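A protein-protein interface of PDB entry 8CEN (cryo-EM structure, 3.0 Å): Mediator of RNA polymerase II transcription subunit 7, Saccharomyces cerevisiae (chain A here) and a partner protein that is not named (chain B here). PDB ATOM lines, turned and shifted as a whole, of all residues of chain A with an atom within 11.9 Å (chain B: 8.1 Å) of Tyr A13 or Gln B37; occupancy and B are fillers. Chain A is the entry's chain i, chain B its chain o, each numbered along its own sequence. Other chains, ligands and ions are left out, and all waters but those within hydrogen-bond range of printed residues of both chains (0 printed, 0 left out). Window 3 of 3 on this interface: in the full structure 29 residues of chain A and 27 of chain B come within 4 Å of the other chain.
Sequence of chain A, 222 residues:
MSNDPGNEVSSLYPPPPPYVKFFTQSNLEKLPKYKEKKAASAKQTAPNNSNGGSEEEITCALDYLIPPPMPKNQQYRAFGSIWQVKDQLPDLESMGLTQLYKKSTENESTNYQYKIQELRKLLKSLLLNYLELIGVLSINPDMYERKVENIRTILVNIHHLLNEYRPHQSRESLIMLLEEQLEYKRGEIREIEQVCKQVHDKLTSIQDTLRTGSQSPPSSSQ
The backbone carbonyl oxygen (O) of Tyr B41 sits at hydrogen-bond distance from the side-chain hydroxyl (OG1) of Thr B44, 3.1 Å away. NE2 of Gln B45 lies within hydrogen-bond range of OH of Tyr B41 (3.1 Å). OD1 of Asn B35 sits close to N of Gln B37 (3.4 Å).
The side-chain hydroxyl (OH) of Tyr B41 sits at hydrogen-bond distance from the side-chain hydroxyl (OG) of Ser A11, 2.5 Å away. The backbone carbonyl oxygen (O) of Pro A14 lies within hydrogen-bond range of the side-chain hydroxyl (OH) of Tyr B38 (2.9 Å).
Ser A10 touches none of the printed residues of chain B. Of the printed residues of chain B, Ser A11 touches Tyr B41 (2.5 Å). Of chain B, only Gln B37, Tyr B38 and Tyr B41 come within 4 Å of Tyr A13. Of the printed residues of chain B, Pro A15 touches Tyr B38 (3.6 Å). Of the printed residues of chain B, Pro A16 touches Tyr B38 and Leu B42. No residue of chain A comes within 4 Å of Asn B35. No residue of chain A comes within 4 Å of Ile B36. Of chain A, only Tyr A13 comes within 4 Å of Gln B37. Of chain A, only Tyr A13, Pro A14, Pro A15 and Pro A16 come within 4 Å of Tyr B38. No residue of chain A comes within 4 Å of Val B39. Tyr B41 touches just these residues of chain A: Ser A11 and Tyr A13. The nearest residue of chain B that does not touch Tyr A13 is Asn B35 (4.1 Å). The nearest residue of chain A that does not touch Gln B37 is Leu A12 (5.9 Å). The nearest printed residue of chain B that does not touch Pro A15 is Leu B42 (5.1 Å).
Among the printed residues, no Asp or Glu carboxylate lies within 4 Å of a Lys or Arg side-chain nitrogen of the other chain.
Among the printed residues, merely in contact across the chains: Tyr A13 with Gln B37, Tyr A13 with Tyr B38, Tyr A13 with Tyr B41, Pro A15 with Tyr B38, Pro A16 with Tyr B38 and Pro A16 with Leu B42.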
ATOM      1  N   VAL A   9      26.578   0.931  -4.601  1.00  0.00           N
ATOM      2  CA  VAL A   9      25.409   1.675  -5.049  1.00  0.00           C
ATOM      3  C   VAL A   9      25.804   3.124  -5.316  1.00  0.00           C
ATOM      4  O   VAL A   9      25.661   3.988  -4.451  1.00  0.00           O
ATOM      5  CB  VAL A   9      24.267   1.590  -4.021  1.00  0.00           C
ATOM      6  CG1 VAL A   9      22.968   2.117  -4.614  1.00  0.00           C
ATOM      7  CG2 VAL A   9      24.100   0.160  -3.529  1.00  0.00           C
ATOM      8  N   SER A  10      26.308   3.382  -6.517  1.00  0.00           N
ATOM      9  CA  SER A  10      26.781   4.702  -6.914  1.00  0.00           C
ATOM     10  C   SER A  10      25.968   5.197  -8.109  1.00  0.00           C
ATOM     11  O   SER A  10      24.962   4.599  -8.499  1.00  0.00           O
ATOM     12  CB  SER A  10      28.278   4.665  -7.227  1.00  0.00           C
ATOM     13  OG  SER A  10      28.538   3.912  -8.399  1.00  0.00           O
ATOM     14  N   SER A  11      26.406   6.314  -8.682  1.00  0.00           N
ATOM     15  CA  SER A  11      25.726   6.879  -9.834  1.00  0.00           C
ATOM     16  C   SER A  11      25.999   6.048 -11.085  1.00  0.00           C
ATOM     17  O   SER A  11      26.939   5.251 -11.145  1.00  0.00           O
ATOM     18  CB  SER A  11      26.165   8.325 -10.059  1.00  0.00           C
ATOM     19  OG  SER A  11      25.562   8.864 -11.222  1.00  0.00           O
ATOM     20  N   LEU A  12      25.148   6.241 -12.093  1.00  0.00           N
ATOM     21  CA  LEU A  12      25.307   5.512 -13.347  1.00  0.00           C
ATOM     22  C   LEU A  12      26.492   6.030 -14.148  1.00  0.00           C
ATOM     23  O   LEU A  12      27.279   5.243 -14.685  1.00  0.00           O
ATOM     24  CB  LEU A  12      24.029   5.612 -14.174  1.00  0.00           C
ATOM     25  CG  LEU A  12      23.870   4.672 -15.370  1.00  0.00           C
ATOM     26  CD1 LEU A  12      23.377   3.306 -14.930  1.00  0.00           C
ATOM     27  CD2 LEU A  12      22.959   5.264 -16.436  1.00  0.00           C
ATOM     28  N   TYR A  13      26.646   7.342 -14.227  1.00  0.00           N
ATOM     29  CA  TYR A  13      27.615   7.927 -15.131  1.00  0.00           C
ATOM     30  C   TYR A  13      28.802   8.505 -14.366  1.00  0.00           C
ATOM     31  O   TYR A  13      28.652   8.952 -13.224  1.00  0.00           O
ATOM     32  CB  TYR A  13      26.963   9.034 -15.966  1.00  0.00           C
ATOM     33  CG  TYR A  13      26.014   8.523 -17.025  1.00  0.00           C
ATOM     34  CD1 TYR A  13      26.447   7.639 -18.003  1.00  0.00           C
ATOM     35  CD2 TYR A  13      24.686   8.925 -17.046  1.00  0.00           C
ATOM     36  CE1 TYR A  13      25.583   7.172 -18.975  1.00  0.00           C
ATOM     37  CE2 TYR A  13      23.815   8.464 -18.014  1.00  0.00           C
ATOM     38  CZ  TYR A  13      24.270   7.587 -18.975  1.00  0.00           C
ATOM     39  OH  TYR A  13      23.408   7.122 -19.941  1.00  0.00           O
ATOM     40  N   PRO A  14      29.997   8.493 -14.962  1.00  0.00           N
ATOM     41  CA  PRO A  14      31.136   9.141 -14.317  1.00  0.00           C
ATOM     42  C   PRO A  14      30.960  10.648 -14.296  1.00  0.00           C
ATOM     43  O   PRO A  14      30.290  11.221 -15.171  1.00  0.00           O
ATOM     44  CB  PRO A  14      32.327   8.728 -15.202  1.00  0.00           C
ATOM     45  CG  PRO A  14      31.857   7.527 -15.948  1.00  0.00           C
ATOM     46  CD  PRO A  14      30.396   7.744 -16.165  1.00  0.00           C
ATOM     47  N   PRO A  15      31.539  11.333 -13.315  1.00  0.00           N
ATOM     48  CA  PRO A  15      31.454  12.795 -13.274  1.00  0.00           C
ATOM     49  C   PRO A  15      32.372  13.425 -14.305  1.00  0.00           C
ATOM     50  O   PRO A  15      33.184  12.726 -14.931  1.00  0.00           O
ATOM     51  CB  PRO A  15      31.904  13.128 -11.842  1.00  0.00           C
ATOM     52  CG  PRO A  15      32.765  11.994 -11.451  1.00  0.00           C
ATOM     53  CD  PRO A  15      32.174  10.782 -12.106  1.00  0.00           C
ATOM     54  N   PRO A  16      32.262  14.734 -14.528  1.00  0.00           N
ATOM     55  CA  PRO A  16      33.248  15.442 -15.358  1.00  0.00           C
ATOM     56  C   PRO A  16      34.635  15.385 -14.739  1.00  0.00           C
ATOM     57  O   PRO A  16      34.772  15.103 -13.538  1.00  0.00           O
ATOM     58  CB  PRO A  16      32.702  16.878 -15.385  1.00  0.00           C
ATOM     59  CG  PRO A  16      31.243  16.703 -15.265  1.00  0.00           C
ATOM     60  CD  PRO A  16      31.059  15.558 -14.307  1.00  0.00           C
ATOM     61  N   PRO A  17      35.691  15.621 -15.529  1.00  0.00           N
ATOM     62  CA  PRO A  17      37.047  15.485 -14.996  1.00  0.00           C
ATOM     63  C   PRO A  17      37.337  16.531 -13.936  1.00  0.00           C
ATOM     64  O   PRO A  17      36.839  17.669 -14.011  1.00  0.00           O
ATOM     65  CB  PRO A  17      37.937  15.686 -16.236  1.00  0.00           C
ATOM     66  CG  PRO A  17      37.062  15.403 -17.391  1.00  0.00           C
ATOM     67  CD  PRO A  17      35.703  15.861 -16.984  1.00  0.00           C
ATOM     68  N   PHE A  79      37.964   4.124 -23.391  1.00  0.00           N
ATOM     69  CA  PHE A  79      36.824   3.203 -23.328  1.00  0.00           C
ATOM     70  C   PHE A  79      37.270   1.748 -23.193  1.00  0.00           C
ATOM     71  O   PHE A  79      36.664   0.838 -23.762  1.00  0.00           O
ATOM     72  CB  PHE A  79      35.902   3.384 -24.535  1.00  0.00           C
ATOM     73  CG  PHE A  79      35.620   4.821 -24.862  1.00  0.00           C
ATOM     74  CD1 PHE A  79      34.901   5.617 -23.986  1.00  0.00           C
ATOM     75  CD2 PHE A  79      36.085   5.380 -26.040  1.00  0.00           C
ATOM     76  CE1 PHE A  79      34.648   6.944 -24.283  1.00  0.00           C
ATOM     77  CE2 PHE A  79      35.834   6.703 -26.343  1.00  0.00           C
ATOM     78  CZ  PHE A  79      35.114   7.486 -25.463  1.00  0.00           C
ATOM     79  N   SER B  32      32.255  11.629 -24.716  1.00  0.00           N
ATOM     80  CA  SER B  32      31.027  11.315 -23.997  1.00  0.00           C
ATOM     81  C   SER B  32      29.900  12.305 -24.271  1.00  0.00           C
ATOM     82  O   SER B  32      28.746  12.003 -23.951  1.00  0.00           O
ATOM     83  CB  SER B  32      31.312  11.260 -22.498  1.00  0.00           C
ATOM     84  OG  SER B  32      31.724  12.527 -22.019  1.00  0.00           O
ATOM     85  N   LEU B  33      30.201  13.472 -24.847  1.00  0.00           N
ATOM     86  CA  LEU B  33      29.161  14.424 -25.219  1.00  0.00           C
ATOM     87  C   LEU B  33      28.285  13.912 -26.354  1.00  0.00           C
ATOM     88  O   LEU B  33      27.160  14.398 -26.516  1.00  0.00           O
ATOM     89  CB  LEU B  33      29.791  15.765 -25.600  1.00  0.00           C
ATOM     90  CG  LEU B  33      29.812  16.853 -24.520  1.00  0.00           C
ATOM     91  CD1 LEU B  33      30.598  16.418 -23.294  1.00  0.00           C
ATOM     92  CD2 LEU B  33      30.380  18.144 -25.079  1.00  0.00           C
ATOM     93  N   ALA B  34      28.775  12.956 -27.151  1.00  0.00           N
ATOM     94  CA  ALA B  34      27.920  12.303 -28.136  1.00  0.00           C
ATOM     95  C   ALA B  34      26.810  11.519 -27.454  1.00  0.00           C
ATOM     96  O   ALA B  34      25.674  11.480 -27.943  1.00  0.00           O
ATOM     97  CB  ALA B  34      28.748  11.383 -29.031  1.00  0.00           C
ATOM     98  N   ASN B  35      27.123  10.877 -26.332  1.00  0.00           N
ATOM     99  CA  ASN B  35      26.096  10.270 -25.495  1.00  0.00           C
ATOM    100  C   ASN B  35      25.296  11.392 -24.856  1.00  0.00           C
ATOM    101  O   ASN B  35      25.770  12.057 -23.931  1.00  0.00           O
ATOM    102  CB  ASN B  35      26.732   9.365 -24.443  1.00  0.00           C
ATOM    103  CG  ASN B  35      25.728   8.434 -23.786  1.00  0.00           C
ATOM    104  OD1 ASN B  35      24.524   8.531 -24.018  1.00  0.00           O
ATOM    105  ND2 ASN B  35      26.225   7.520 -22.964  1.00  0.00           N
ATOM    106  N   ILE B  36      24.090  11.627 -25.370  1.00  0.00           N
ATOM    107  CA  ILE B  36      23.282  12.738 -24.900  1.00  0.00           C
ATOM    108  C   ILE B  36      22.270  12.319 -23.851  1.00  0.00           C
ATOM    109  O   ILE B  36      21.466  13.148 -23.407  1.00  0.00           O
ATOM    110  CB  ILE B  36      22.617  13.465 -26.084  1.00  0.00           C
ATOM    111  CG1 ILE B  36      21.680  12.537 -26.839  1.00  0.00           C
ATOM    112  CG2 ILE B  36      23.672  14.032 -27.021  1.00  0.00           C
ATOM    113  CD1 ILE B  36      20.868  13.275 -27.836  1.00  0.00           C
ATOM    114  N   GLN B  37      22.285  11.051 -23.440  1.00  0.00           N
ATOM    115  CA  GLN B  37      21.814  10.714 -22.105  1.00  0.00           C
ATOM    116  C   GLN B  37      22.810  11.183 -21.054  1.00  0.00           C
ATOM    117  O   GLN B  37      22.415  11.601 -19.959  1.00  0.00           O
ATOM    118  CB  GLN B  37      21.590   9.208 -21.984  1.00  0.00           C
ATOM    119  CG  GLN B  37      20.261   8.723 -22.524  1.00  0.00           C
ATOM    120  CD  GLN B  37      19.996   7.272 -22.182  1.00  0.00           C
ATOM    121  OE1 GLN B  37      19.615   6.947 -21.057  1.00  0.00           O
ATOM    122  NE2 GLN B  37      20.198   6.389 -23.151  1.00  0.00           N
ATOM    123  N   TYR B  38      24.105  11.135 -21.384  1.00  0.00           N
ATOM    124  CA  TYR B  38      25.137  11.558 -20.444  1.00  0.00           C
ATOM    125  C   TYR B  38      25.124  13.067 -20.234  1.00  0.00           C
ATOM    126  O   TYR B  38      25.268  13.535 -19.099  1.00  0.00           O
ATOM    127  CB  TYR B  38      26.512  11.106 -20.928  1.00  0.00           C
ATOM    128  CG  TYR B  38      27.632  11.568 -20.032  1.00  0.00           C
ATOM    129  CD1 TYR B  38      27.708  11.145 -18.716  1.00  0.00           C
ATOM    130  CD2 TYR B  38      28.596  12.449 -20.493  1.00  0.00           C
ATOM    131  CE1 TYR B  38      28.724  11.569 -17.890  1.00  0.00           C
ATOM    132  CE2 TYR B  38      29.618  12.881 -19.674  1.00  0.00           C
ATOM    133  CZ  TYR B  38      29.677  12.437 -18.372  1.00  0.00           C
ATOM    134  OH  TYR B  38      30.692  12.864 -17.550  1.00  0.00           O
ATOM    135  N   VAL B  39      24.958  13.852 -21.301  1.00  0.00           N
ATOM    136  CA  VAL B  39      24.890  15.295 -21.085  1.00  0.00           C
ATOM    137  C   VAL B  39      23.552  15.690 -20.480  1.00  0.00           C
ATOM    138  O   VAL B  39      23.472  16.725 -19.817  1.00  0.00           O
ATOM    139  CB  VAL B  39      25.145  16.124 -22.358  1.00  0.00           C
ATOM    140  CG1 VAL B  39      26.541  15.861 -22.902  1.00  0.00           C
ATOM    141  CG2 VAL B  39      24.073  15.911 -23.403  1.00  0.00           C
ATOM    142  N   THR B  40      22.506  14.878 -20.663  1.00  0.00           N
ATOM    143  CA  THR B  40      21.278  15.080 -19.902  1.00  0.00           C
ATOM    144  C   THR B  40      21.524  14.874 -18.413  1.00  0.00           C
ATOM    145  O   THR B  40      21.068  15.669 -17.585  1.00  0.00           O
ATOM    146  CB  THR B  40      20.186  14.133 -20.399  1.00  0.00           C
ATOM    147  OG1 THR B  40      20.092  14.216 -21.826  1.00  0.00           O
ATOM    148  CG2 THR B  40      18.842  14.497 -19.787  1.00  0.00           C
ATOM    149  N   TYR B  41      22.274  13.826 -18.061  1.00  0.00           N
ATOM    150  CA  TYR B  41      22.643  13.597 -16.666  1.00  0.00           C
ATOM    151  C   TYR B  41      23.507  14.732 -16.125  1.00  0.00           C
ATOM    152  O   TYR B  41      23.373  15.124 -14.959  1.00  0.00           O
ATOM    153  CB  TYR B  41      23.368  12.256 -16.543  1.00  0.00           C
ATOM    154  CG  TYR B  41      24.053  12.020 -15.215  1.00  0.00           C
ATOM    155  CD1 TYR B  41      23.329  11.637 -14.094  1.00  0.00           C
ATOM    156  CD2 TYR B  41      25.430  12.163 -15.090  1.00  0.00           C
ATOM    157  CE1 TYR B  41      23.957  11.414 -12.884  1.00  0.00           C
ATOM    158  CE2 TYR B  41      26.065  11.943 -13.886  1.00  0.00           C
ATOM    159  CZ  TYR B  41      25.324  11.568 -12.787  1.00  0.00           C
ATOM    160  OH  TYR B  41      25.956  11.348 -11.586  1.00  0.00           O
ATOM    161  N   LEU B  42      24.406  15.262 -16.955  1.00  0.00           N
ATOM    162  CA  LEU B  42      25.262  16.365 -16.528  1.00  0.00           C
ATOM    163  C   LEU B  42      24.466  17.650 -16.327  1.00  0.00           C
ATOM    164  O   LEU B  42      24.665  18.361 -15.336  1.00  0.00           O
ATOM    165  CB  LEU B  42      26.375  16.595 -17.549  1.00  0.00           C
ATOM    166  CG  LEU B  42      27.497  15.565 -17.661  1.00  0.00           C
ATOM    167  CD1 LEU B  42      28.662  16.158 -18.434  1.00  0.00           C
ATOM    168  CD2 LEU B  42      27.943  15.090 -16.291  1.00  0.00           C
ATOM    169  N   LEU B  43      23.558  17.960 -17.247  1.00  0.00           N
ATOM    170  CA  LEU B  43      22.828  19.216 -17.236  1.00  0.00           C
ATOM    171  C   LEU B  43      21.508  19.130 -16.482  1.00  0.00           C
ATOM    172  O   LEU B  43      20.728  20.084 -16.521  1.00  0.00           O
ATOM    173  CB  LEU B  43      22.586  19.691 -18.671  1.00  0.00           C
ATOM    174  CG  LEU B  43      23.856  19.954 -19.486  1.00  0.00           C
ATOM    175  CD1 LEU B  43      23.522  20.566 -20.830  1.00  0.00           C
ATOM    176  CD2 LEU B  43      24.828  20.839 -18.718  1.00  0.00           C
ATOM    177  N   THR B  44      21.215  18.000 -15.844  1.00  0.00           N
ATOM    178  CA  THR B  44      20.150  17.945 -14.853  1.00  0.00           C
ATOM    179  C   THR B  44      20.656  18.101 -13.424  1.00  0.00           C
ATOM    180  O   THR B  44      19.853  18.042 -12.489  1.00  0.00           O
ATOM    181  CB  THR B  44      19.362  16.638 -14.981  1.00  0.00           C
ATOM    182  OG1 THR B  44      20.265  15.536 -15.136  1.00  0.00           O
ATOM    183  CG2 THR B  44      18.392  16.703 -16.154  1.00  0.00           C
ATOM    184  N   GLN B  45      21.959  18.290 -13.230  1.00  0.00           N
ATOM    185  CA  GLN B  45      22.511  18.577 -11.912  1.00  0.00           C
ATOM    186  C   GLN B  45      22.716  20.080 -11.778  1.00  0.00           C
ATOM    187  O   GLN B  45      23.394  20.694 -12.609  1.00  0.00           O
ATOM    188  CB  GLN B  45      23.821  17.825 -11.688  1.00  0.00           C
ATOM    189  CG  GLN B  45      23.653  16.320 -11.613  1.00  0.00           C
ATOM    190  CD  GLN B  45      24.965  15.595 -11.404  1.00  0.00           C
ATOM    191  OE1 GLN B  45      26.029  16.210 -11.378  1.00  0.00           O
ATOM    192  NE2 GLN B  45      24.894  14.283 -11.234  1.00  0.00           N
ATOM    193  N   ILE B 110      17.534  20.558 -23.385  1.00  0.00           N
ATOM    194  CA  ILE B 110      18.175  19.247 -23.476  1.00  0.00           C
ATOM    195  C   ILE B 110      17.166  18.131 -23.232  1.00  0.00           C
ATOM    196  O   ILE B 110      17.095  17.167 -23.999  1.00  0.00           O
ATOM    197  CB  ILE B 110      19.369  19.147 -22.509  1.00  0.00           C
ATOM    198  CG1 ILE B 110      20.414  20.219 -22.818  1.00  0.00           C
ATOM    199  CG2 ILE B 110      20.001  17.764 -22.574  1.00  0.00           C
ATOM    200  CD1 ILE B 110      21.009  20.121 -24.198  1.00  0.00           C
ATOM    201  N   GLY B 114      16.391  15.910 -26.477  1.00  0.00           N
ATOM    202  CA  GLY B 114      17.294  14.786 -26.414  1.00  0.00           C
ATOM    203  C   GLY B 114      16.911  13.607 -27.286  1.00  0.00           C
ATOM    204  O   GLY B 114      17.702  13.162 -28.128  1.00  0.00           O
ATOM    205  N   PRO B 115      15.705  13.050 -27.081  1.00  0.00           N
ATOM    206  CA  PRO B 115      15.246  11.967 -27.970  1.00  0.00           C
ATOM    207  C   PRO B 115      15.239  12.341 -29.441  1.00  0.00           C
ATOM    208  O   PRO B 115      15.612  11.516 -30.283  1.00  0.00           O
ATOM    209  CB  PRO B 115      13.834  11.676 -27.446  1.00  0.00           C
ATOM    210  CG  PRO B 115      13.920  11.987 -26.003  1.00  0.00           C
ATOM    211  CD  PRO B 115      14.842  13.170 -25.890  1.00  0.00           C
ATOM    212  N   MET B 118      19.012  12.409 -30.668  1.00  0.00           N
ATOM    213  CA  MET B 118      19.596  11.085 -30.842  1.00  0.00           C
ATOM    214  C   MET B 118      18.894  10.312 -31.949  1.00  0.00           C
ATOM    215  O   MET B 118      19.536   9.516 -32.641  1.00  0.00           O
ATOM    216  CB  MET B 118      19.593  10.297 -29.531  1.00  0.00           C
ATOM    217  CG  MET B 118      18.252  10.056 -28.898  1.00  0.00           C
ATOM    218  SD  MET B 118      18.487   9.535 -27.192  1.00  0.00           S
ATOM    219  CE  MET B 118      19.597   8.152 -27.437  1.00  0.00           C
